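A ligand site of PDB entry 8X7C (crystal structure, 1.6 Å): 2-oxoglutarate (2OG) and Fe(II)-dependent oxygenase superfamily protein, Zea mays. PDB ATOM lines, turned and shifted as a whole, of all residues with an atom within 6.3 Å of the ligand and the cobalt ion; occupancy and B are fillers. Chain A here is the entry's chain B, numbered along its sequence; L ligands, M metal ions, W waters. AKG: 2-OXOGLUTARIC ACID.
Three residues have an atom within 4 Å of the cobalt ion: His 228, Asp 230 and His 285. Along chain A the residues within 4 Å of the cobalt ion span positions 228 to 285.
An oxygen (O4) of the ligand lies within hydrogen-bond range of the side-chain hydroxyl of Tyr 213, at 2.6 Å. The guanidinium group of Arg 209 is in salt-bridge range of an oxygen (O2) of the ligand (3.5 Å). The side-chain amide nitrogen (ND2) of Asn 211 is in hydrogen-bond range of an oxygen (O2) of the ligand (3.1 Å). An oxygen (O3) of the ligand lies within salt-bridge range of the guanidinium group (NH2) of Arg 295 (2.8 Å). The side-chain hydroxyl of Ser 297 lies within hydrogen-bond range of an oxygen (O4) of the ligand (2.7 Å).
The cobalt ion is bound by O1 of the ligand, NE2 of His 228, water W3, O5 of the ligand, NE2 of His 285 and OD1 of Asp 230. The cobalt ion has six donor atoms within binding distance.
CD1 of Ile 225 touches C1 of the ligand, 3.8 Å away. Leu 237 touches the ligand (CD2 to O3, 3.4 Å). Leu 246 touches the ligand (CD1 to O3, 3.7 Å). Val 287 touches the ligand (CG2 to C5, 3.5 Å). Ala 299 touches the ligand (CB to O2, 3.9 Å). Phe 301 touches the ligand (CZ to O1, 3.3 Å). Hydrophobic or aromatic side chains that line the ligand: Tyr 213, Ile 225, His 228, Leu 237, Leu 246, His 285, Val 287, Ala 299 and Phe 301. Along chain A the residues within 4 Å of the ligand span positions 209 to 301.
The backbone NH (N) of Val 287 sits at hydrogen-bond distance from the backbone carbonyl oxygen (O) of Ile 225 (3.1 Å). The side-chain carboxylate (OD2) of Asp 230 lies within hydrogen-bond range of the side-chain amide nitrogen (ND2) of Asn 267. NH2 of Arg 209 lies within hydrogen-bond range of OE1 of Gln 138 (3.0 Å). The backbone carbonyl oxygen of Arg 295 is in hydrogen-bond range of the backbone NH of Tyr 213 (2.8 Å). The side-chain carboxylate of Asp 230 sits at hydrogen-bond distance from the side-chain hydroxyl of Thr 235. O of Ala 299 sits at hydrogen-bond distance from N of Arg 209. The side-chain amide oxygen (OD1) of Asn 211 is in hydrogen-bond range of the side-chain amide nitrogen (NE2) of Gln 138 (2.8 Å). The side-chain amide oxygen of Asn 211 lies within hydrogen-bond range of the guanidinium group of Arg 209 (2.8 Å).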
ATOM      1  N   GLN A 138      -9.896 -12.522   6.193  1.00  0.00           N
ATOM      2  CA  GLN A 138     -11.011 -13.243   6.805  1.00  0.00           C
ATOM      3  C   GLN A 138     -12.275 -12.970   6.019  1.00  0.00           C
ATOM      4  O   GLN A 138     -12.371 -11.975   5.287  1.00  0.00           O
ATOM      5  CB  GLN A 138     -11.226 -12.854   8.276  1.00  0.00           C
ATOM      6  CG  GLN A 138     -11.903 -11.486   8.454  1.00  0.00           C
ATOM      7  CD  GLN A 138     -12.744 -11.395   9.728  1.00  0.00           C
ATOM      8  OE1 GLN A 138     -12.656 -10.417  10.476  1.00  0.00           O
ATOM      9  NE2 GLN A 138     -13.557 -12.407   9.991  1.00  0.00           N
ATOM     10  N   ARG A 209     -21.391 -13.096  15.081  1.00  0.00           N
ATOM     11  CA  ARG A 209     -20.418 -12.950  13.992  1.00  0.00           C
ATOM     12  C   ARG A 209     -19.594 -14.229  13.901  1.00  0.00           C
ATOM     13  O   ARG A 209     -18.801 -14.527  14.805  1.00  0.00           O
ATOM     14  CB  ARG A 209     -19.533 -11.734  14.214  1.00  0.00           C
ATOM     15  CG  ARG A 209     -18.531 -11.511  13.075  1.00  0.00           C
ATOM     16  CD  ARG A 209     -17.658 -10.289  13.375  1.00  0.00           C
ATOM     17  NE  ARG A 209     -16.550 -10.172  12.418  1.00  0.00           N
ATOM     18  CZ  ARG A 209     -16.432  -9.217  11.500  1.00  0.00           C
ATOM     19  NH1 ARG A 209     -17.356  -8.260  11.417  1.00  0.00           N
ATOM     20  NH2 ARG A 209     -15.378  -9.203  10.687  1.00  0.00           N
ATOM     21  N   ASN A 211     -16.627 -15.835  12.261  1.00  0.00           N
ATOM     22  CA  ASN A 211     -15.408 -15.477  11.543  1.00  0.00           C
ATOM     23  C   ASN A 211     -14.747 -16.699  10.947  1.00  0.00           C
ATOM     24  O   ASN A 211     -14.609 -17.728  11.626  1.00  0.00           O
ATOM     25  CB  ASN A 211     -14.406 -14.817  12.492  1.00  0.00           C
ATOM     26  CG  ASN A 211     -14.905 -13.490  13.016  1.00  0.00           C
ATOM     27  OD1 ASN A 211     -15.155 -12.560  12.250  1.00  0.00           O
ATOM     28  ND2 ASN A 211     -15.044 -13.383  14.341  1.00  0.00           N
ATOM     29  N   TYR A 213     -11.106 -17.538   9.106  1.00  0.00           N
ATOM     30  CA  TYR A 213      -9.783 -17.054   8.709  1.00  0.00           C
ATOM     31  C   TYR A 213      -9.098 -18.126   7.883  1.00  0.00           C
ATOM     32  O   TYR A 213      -8.691 -19.142   8.452  1.00  0.00           O
ATOM     33  CB  TYR A 213      -8.919 -16.708   9.928  1.00  0.00           C
ATOM     34  CG  TYR A 213      -9.577 -15.779  10.897  1.00  0.00           C
ATOM     35  CD1 TYR A 213      -9.395 -14.413  10.816  1.00  0.00           C
ATOM     36  CD2 TYR A 213     -10.405 -16.289  11.909  1.00  0.00           C
ATOM     37  CE1 TYR A 213     -10.025 -13.539  11.734  1.00  0.00           C
ATOM     38  CE2 TYR A 213     -11.042 -15.421  12.812  1.00  0.00           C
ATOM     39  CZ  TYR A 213     -10.843 -14.066  12.722  1.00  0.00           C
ATOM     40  OH  TYR A 213     -11.463 -13.209  13.615  1.00  0.00           O
ATOM     41  N   ILE A 225      -7.998 -10.298  11.652  1.00  0.00           N
ATOM     42  CA  ILE A 225      -8.875  -9.157  11.899  1.00  0.00           C
ATOM     43  C   ILE A 225      -8.012  -8.064  12.500  1.00  0.00           C
ATOM     44  O   ILE A 225      -7.160  -8.333  13.367  1.00  0.00           O
ATOM     45  CB  ILE A 225     -10.104  -9.514  12.775  1.00  0.00           C
ATOM     46  CG1 ILE A 225     -11.196  -8.454  12.673  1.00  0.00           C
ATOM     47  CG2 ILE A 225      -9.767  -9.748  14.237  1.00  0.00           C
ATOM     48  CD1 ILE A 225     -12.534  -8.872  13.319  1.00  0.00           C
ATOM     49  N   HIS A 228      -8.817  -3.625  16.863  1.00  0.00           N
ATOM     50  CA  HIS A 228     -10.067  -2.922  17.077  1.00  0.00           C
ATOM     51  C   HIS A 228     -10.494  -3.160  18.503  1.00  0.00           C
ATOM     52  O   HIS A 228     -10.007  -4.076  19.151  1.00  0.00           O
ATOM     53  CB  HIS A 228     -11.160  -3.433  16.117  1.00  0.00           C
ATOM     54  CG  HIS A 228     -11.588  -4.849  16.413  1.00  0.00           C
ATOM     55  ND1 HIS A 228     -10.869  -5.948  15.998  1.00  0.00           N
ATOM     56  CD2 HIS A 228     -12.656  -5.330  17.091  1.00  0.00           C
ATOM     57  CE1 HIS A 228     -11.472  -7.047  16.416  1.00  0.00           C
ATOM     58  NE2 HIS A 228     -12.566  -6.694  17.078  1.00  0.00           N
ATOM     59  N   SER A 229     -11.423  -2.342  18.979  1.00  0.00           N
ATOM     60  CA  SER A 229     -12.210  -2.708  20.151  1.00  0.00           C
ATOM     61  C   SER A 229     -13.646  -2.902  19.696  1.00  0.00           C
ATOM     62  O   SER A 229     -14.081  -2.325  18.687  1.00  0.00           O
ATOM     63  CB  SER A 229     -12.122  -1.657  21.259  1.00  0.00           C
ATOM     64  OG  SER A 229     -12.570  -0.384  20.803  1.00  0.00           O
ATOM     65  N   ASP A 230     -14.373  -3.757  20.409  1.00  0.00           N
ATOM     66  CA  ASP A 230     -15.780  -3.982  20.074  1.00  0.00           C
ATOM     67  C   ASP A 230     -16.609  -2.807  20.601  1.00  0.00           C
ATOM     68  O   ASP A 230     -16.268  -2.194  21.606  1.00  0.00           O
ATOM     69  CB  ASP A 230     -16.291  -5.291  20.679  1.00  0.00           C
ATOM     70  CG  ASP A 230     -15.533  -6.521  20.197  1.00  0.00           C
ATOM     71  OD1 ASP A 230     -14.889  -6.508  19.124  1.00  0.00           O
ATOM     72  OD2 ASP A 230     -15.614  -7.535  20.927  1.00  0.00           O
ATOM     73  N   THR A 235     -18.758  -8.883  24.903  1.00  0.00           N
ATOM     74  CA  THR A 235     -18.648  -9.884  23.862  1.00  0.00           C
ATOM     75  C   THR A 235     -18.322 -11.233  24.488  1.00  0.00           C
ATOM     76  O   THR A 235     -17.459 -11.313  25.356  1.00  0.00           O
ATOM     77  CB  THR A 235     -17.543  -9.530  22.868  1.00  0.00           C
ATOM     78  OG1 THR A 235     -17.880  -8.271  22.268  1.00  0.00           O
ATOM     79  CG2 THR A 235     -17.392 -10.614  21.767  1.00  0.00           C
ATOM     80  N   LEU A 237     -16.954 -14.868  23.269  1.00  0.00           N
ATOM     81  CA  LEU A 237     -16.220 -15.382  22.104  1.00  0.00           C
ATOM     82  C   LEU A 237     -15.909 -16.865  22.260  1.00  0.00           C
ATOM     83  O   LEU A 237     -15.389 -17.282  23.290  1.00  0.00           O
ATOM     84  CB  LEU A 237     -14.901 -14.604  21.924  1.00  0.00           C
ATOM     85  CG  LEU A 237     -14.041 -15.074  20.748  1.00  0.00           C
ATOM     86  CD1 LEU A 237     -14.635 -14.616  19.406  1.00  0.00           C
ATOM     87  CD2 LEU A 237     -12.618 -14.510  20.918  1.00  0.00           C
ATOM     88  N   LEU A 238     -16.204 -17.633  21.208  1.00  0.00           N
ATOM     89  CA  LEU A 238     -15.878 -19.045  21.109  1.00  0.00           C
ATOM     90  C   LEU A 238     -14.910 -19.248  19.949  1.00  0.00           C
ATOM     91  O   LEU A 238     -15.176 -18.812  18.826  1.00  0.00           O
ATOM     92  CB  LEU A 238     -17.161 -19.866  20.896  1.00  0.00           C
ATOM     93  CG  LEU A 238     -17.036 -21.337  20.519  1.00  0.00           C
ATOM     94  CD1 LEU A 238     -16.350 -22.093  21.654  1.00  0.00           C
ATOM     95  CD2 LEU A 238     -18.435 -21.904  20.259  1.00  0.00           C
ATOM     96  N   VAL A 239     -13.783 -19.904  20.214  1.00  0.00           N
ATOM     97  CA  VAL A 239     -12.790 -20.209  19.176  1.00  0.00           C
ATOM     98  C   VAL A 239     -12.763 -21.708  18.975  1.00  0.00           C
ATOM     99  O   VAL A 239     -12.470 -22.452  19.916  1.00  0.00           O
ATOM    100  CB  VAL A 239     -11.397 -19.694  19.559  1.00  0.00           C
ATOM    101  CG1 VAL A 239     -10.380 -20.065  18.463  1.00  0.00           C
ATOM    102  CG2 VAL A 239     -11.417 -18.183  19.840  1.00  0.00           C
ATOM    103  N   GLY A 245      -4.319 -17.331  17.584  1.00  0.00           N
ATOM    104  CA  GLY A 245      -4.436 -16.198  16.682  1.00  0.00           C
ATOM    105  C   GLY A 245      -4.843 -14.918  17.390  1.00  0.00           C
ATOM    106  O   GLY A 245      -4.380 -13.832  17.006  1.00  0.00           O
ATOM    107  N   LEU A 246      -5.683 -15.021  18.418  1.00  0.00           N
ATOM    108  CA  LEU A 246      -6.179 -13.834  19.102  1.00  0.00           C
ATOM    109  C   LEU A 246      -5.096 -13.221  19.986  1.00  0.00           C
ATOM    110  O   LEU A 246      -4.422 -13.935  20.741  1.00  0.00           O
ATOM    111  CB  LEU A 246      -7.396 -14.190  19.965  1.00  0.00           C
ATOM    112  CG  LEU A 246      -8.033 -13.025  20.713  1.00  0.00           C
ATOM    113  CD1 LEU A 246      -8.666 -12.020  19.746  1.00  0.00           C
ATOM    114  CD2 LEU A 246      -9.072 -13.587  21.671  1.00  0.00           C
ATOM    115  N   ASN A 267     -14.959 -10.302  26.712  1.00  0.00           N
ATOM    116  CA  ASN A 267     -14.289  -9.016  26.708  1.00  0.00           C
ATOM    117  C   ASN A 267     -15.300  -7.874  26.733  1.00  0.00           C
ATOM    118  O   ASN A 267     -16.446  -8.015  26.310  1.00  0.00           O
ATOM    119  CB  ASN A 267     -13.317  -8.863  25.516  1.00  0.00           C
ATOM    120  CG  ASN A 267     -14.009  -8.840  24.179  1.00  0.00           C
ATOM    121  OD1 ASN A 267     -14.178  -9.869  23.540  1.00  0.00           O
ATOM    122  ND2 ASN A 267     -14.393  -7.649  23.733  1.00  0.00           N
ATOM    123  N   HIS A 285      -8.006  -5.564  20.417  1.00  0.00           N
ATOM    124  CA  HIS A 285      -7.570  -6.922  20.134  1.00  0.00           C
ATOM    125  C   HIS A 285      -7.480  -7.120  18.623  1.00  0.00           C
ATOM    126  O   HIS A 285      -7.972  -6.307  17.836  1.00  0.00           O
ATOM    127  CB  HIS A 285      -8.535  -7.930  20.803  1.00  0.00           C
ATOM    128  CG  HIS A 285      -9.987  -7.695  20.497  1.00  0.00           C
ATOM    129  ND1 HIS A 285     -10.732  -6.697  21.090  1.00  0.00           N
ATOM    130  CD2 HIS A 285     -10.828  -8.361  19.667  1.00  0.00           C
ATOM    131  CE1 HIS A 285     -11.965  -6.747  20.629  1.00  0.00           C
ATOM    132  NE2 HIS A 285     -12.063  -7.745  19.774  1.00  0.00           N
ATOM    133  N   ARG A 286      -6.805  -8.188  18.210  1.00  0.00           N
ATOM    134  CA  ARG A 286      -6.594  -8.503  16.799  1.00  0.00           C
ATOM    135  C   ARG A 286      -6.391 -10.006  16.668  1.00  0.00           C
ATOM    136  O   ARG A 286      -6.176 -10.705  17.661  1.00  0.00           O
ATOM    137  CB  ARG A 286      -5.376  -7.752  16.217  1.00  0.00           C
ATOM    138  CG  ARG A 286      -4.045  -8.298  16.744  1.00  0.00           C
ATOM    139  CD  ARG A 286      -2.859  -7.402  16.382  1.00  0.00           C
ATOM    140  NE  ARG A 286      -1.594  -8.067  16.696  1.00  0.00           N
ATOM    141  CZ  ARG A 286      -0.387  -7.509  16.542  1.00  0.00           C
ATOM    142  NH1 ARG A 286      -0.267  -6.273  16.084  1.00  0.00           N
ATOM    143  NH2 ARG A 286       0.706  -8.205  16.858  1.00  0.00           N
ATOM    144  N   VAL A 287      -6.460 -10.492  15.434  1.00  0.00           N
ATOM    145  CA  VAL A 287      -6.156 -11.894  15.139  1.00  0.00           C
ATOM    146  C   VAL A 287      -5.078 -11.942  14.078  1.00  0.00           C
ATOM    147  O   VAL A 287      -5.187 -11.276  13.038  1.00  0.00           O
ATOM    148  CB  VAL A 287      -7.410 -12.678  14.671  1.00  0.00           C
ATOM    149  CG1 VAL A 287      -7.014 -14.034  14.117  1.00  0.00           C
ATOM    150  CG2 VAL A 287      -8.385 -12.860  15.809  1.00  0.00           C
ATOM    151  N   ARG A 295      -8.951 -20.975  10.737  1.00  0.00           N
ATOM    152  CA  ARG A 295      -9.368 -20.725  12.097  1.00  0.00           C
ATOM    153  C   ARG A 295     -10.795 -20.205  12.058  1.00  0.00           C
ATOM    154  O   ARG A 295     -11.130 -19.382  11.197  1.00  0.00           O
ATOM    155  CB  ARG A 295      -8.439 -19.712  12.781  1.00  0.00           C
ATOM    156  CG  ARG A 295      -8.834 -19.318  14.196  1.00  0.00           C
ATOM    157  CD  ARG A 295      -7.819 -18.279  14.718  1.00  0.00           C
ATOM    158  NE  ARG A 295      -8.052 -17.901  16.100  1.00  0.00           N
ATOM    159  CZ  ARG A 295      -8.940 -16.990  16.475  1.00  0.00           C
ATOM    160  NH1 ARG A 295      -9.671 -16.375  15.542  1.00  0.00           N
ATOM    161  NH2 ARG A 295      -9.105 -16.670  17.763  1.00  0.00           N
ATOM    162  N   LEU A 296     -11.634 -20.706  12.957  1.00  0.00           N
ATOM    163  CA  LEU A 296     -13.050 -20.333  13.037  1.00  0.00           C
ATOM    164  C   LEU A 296     -13.379 -19.826  14.433  1.00  0.00           C
ATOM    165  O   LEU A 296     -13.004 -20.441  15.436  1.00  0.00           O
ATOM    166  CB  LEU A 296     -13.970 -21.513  12.723  1.00  0.00           C
ATOM    167  CG  LEU A 296     -14.085 -21.887  11.244  1.00  0.00           C
ATOM    168  CD1 LEU A 296     -12.896 -22.698  10.751  1.00  0.00           C
ATOM    169  CD2 LEU A 296     -15.356 -22.639  10.979  1.00  0.00           C
ATOM    170  N   SER A 297     -14.104 -18.707  14.501  1.00  0.00           N
ATOM    171  CA  SER A 297     -14.579 -18.233  15.786  1.00  0.00           C
ATOM    172  C   SER A 297     -16.008 -17.754  15.637  1.00  0.00           C
ATOM    173  O   SER A 297     -16.491 -17.487  14.528  1.00  0.00           O
ATOM    174  CB  SER A 297     -13.697 -17.094  16.355  1.00  0.00           C
ATOM    175  OG  SER A 297     -13.820 -15.905  15.574  1.00  0.00           O
ATOM    176  N   LEU A 298     -16.686 -17.648  16.780  1.00  0.00           N
ATOM    177  CA  LEU A 298     -18.040 -17.101  16.845  1.00  0.00           C
ATOM    178  C   LEU A 298     -18.063 -16.073  17.964  1.00  0.00           C
ATOM    179  O   LEU A 298     -17.857 -16.428  19.135  1.00  0.00           O
ATOM    180  CB  LEU A 298     -19.067 -18.201  17.102  1.00  0.00           C
ATOM    181  CG  LEU A 298     -20.489 -17.743  17.466  1.00  0.00           C
ATOM    182  CD1 LEU A 298     -21.044 -16.767  16.410  1.00  0.00           C
ATOM    183  CD2 LEU A 298     -21.387 -18.957  17.583  1.00  0.00           C
ATOM    184  N   ALA A 299     -18.299 -14.822  17.610  1.00  0.00           N
ATOM    185  CA  ALA A 299     -18.415 -13.726  18.570  1.00  0.00           C
ATOM    186  C   ALA A 299     -19.881 -13.401  18.757  1.00  0.00           C
ATOM    187  O   ALA A 299     -20.607 -13.194  17.786  1.00  0.00           O
ATOM    188  CB  ALA A 299     -17.663 -12.488  18.079  1.00  0.00           C
ATOM    189  N   PHE A 301     -21.922 -10.500  20.150  1.00  0.00           N
ATOM    190  CA  PHE A 301     -21.816  -9.104  20.567  1.00  0.00           C
ATOM    191  C   PHE A 301     -23.097  -8.703  21.273  1.00  0.00           C
ATOM    192  O   PHE A 301     -24.160  -8.723  20.666  1.00  0.00           O
ATOM    193  CB  PHE A 301     -21.616  -8.177  19.356  1.00  0.00           C
ATOM    194  CG  PHE A 301     -20.400  -8.459  18.533  1.00  0.00           C
ATOM    195  CD1 PHE A 301     -20.508  -8.638  17.156  1.00  0.00           C
ATOM    196  CD2 PHE A 301     -19.137  -8.500  19.122  1.00  0.00           C
ATOM    197  CE1 PHE A 301     -19.380  -8.875  16.374  1.00  0.00           C
ATOM    198  CE2 PHE A 301     -18.002  -8.752  18.329  1.00  0.00           C
ATOM    199  CZ  PHE A 301     -18.136  -8.923  16.961  1.00  0.00           C
HETATM  200  C1  AKG L   1     -14.541  -9.876  16.410  1.00  0.00           C
HETATM  201  O1  AKG L   1     -14.833  -8.716  16.773  1.00  0.00           O
HETATM  202  O2  AKG L   1     -15.266 -10.579  15.637  1.00  0.00           O
HETATM  203  C2  AKG L   1     -13.264 -10.479  16.943  1.00  0.00           C
HETATM  204  O5  AKG L   1     -12.543  -9.785  17.615  1.00  0.00           O
HETATM  205  C3  AKG L   1     -12.938 -11.941  16.582  1.00  0.00           C
HETATM  206  C4  AKG L   1     -11.796 -12.405  17.476  1.00  0.00           C
HETATM  207  C5  AKG L   1     -11.430 -13.831  17.109  1.00  0.00           C
HETATM  208  O3  AKG L   1     -10.859 -14.492  17.997  1.00  0.00           O
HETATM  209  O4  AKG L   1     -11.675 -14.345  15.977  1.00  0.00           O
HETATM  210 CO    CO M   1     -13.589  -8.061  18.301  1.00  0.00          CO
HETATM  211  O   HOH W   1     -15.950  -7.252  14.872  1.00  0.00           O
HETATM  212  O   HOH W   2     -16.163  -5.565  16.771  1.00  0.00           O
HETATM  213  O   HOH W   3     -14.497  -9.465  19.581  1.00  0.00           O
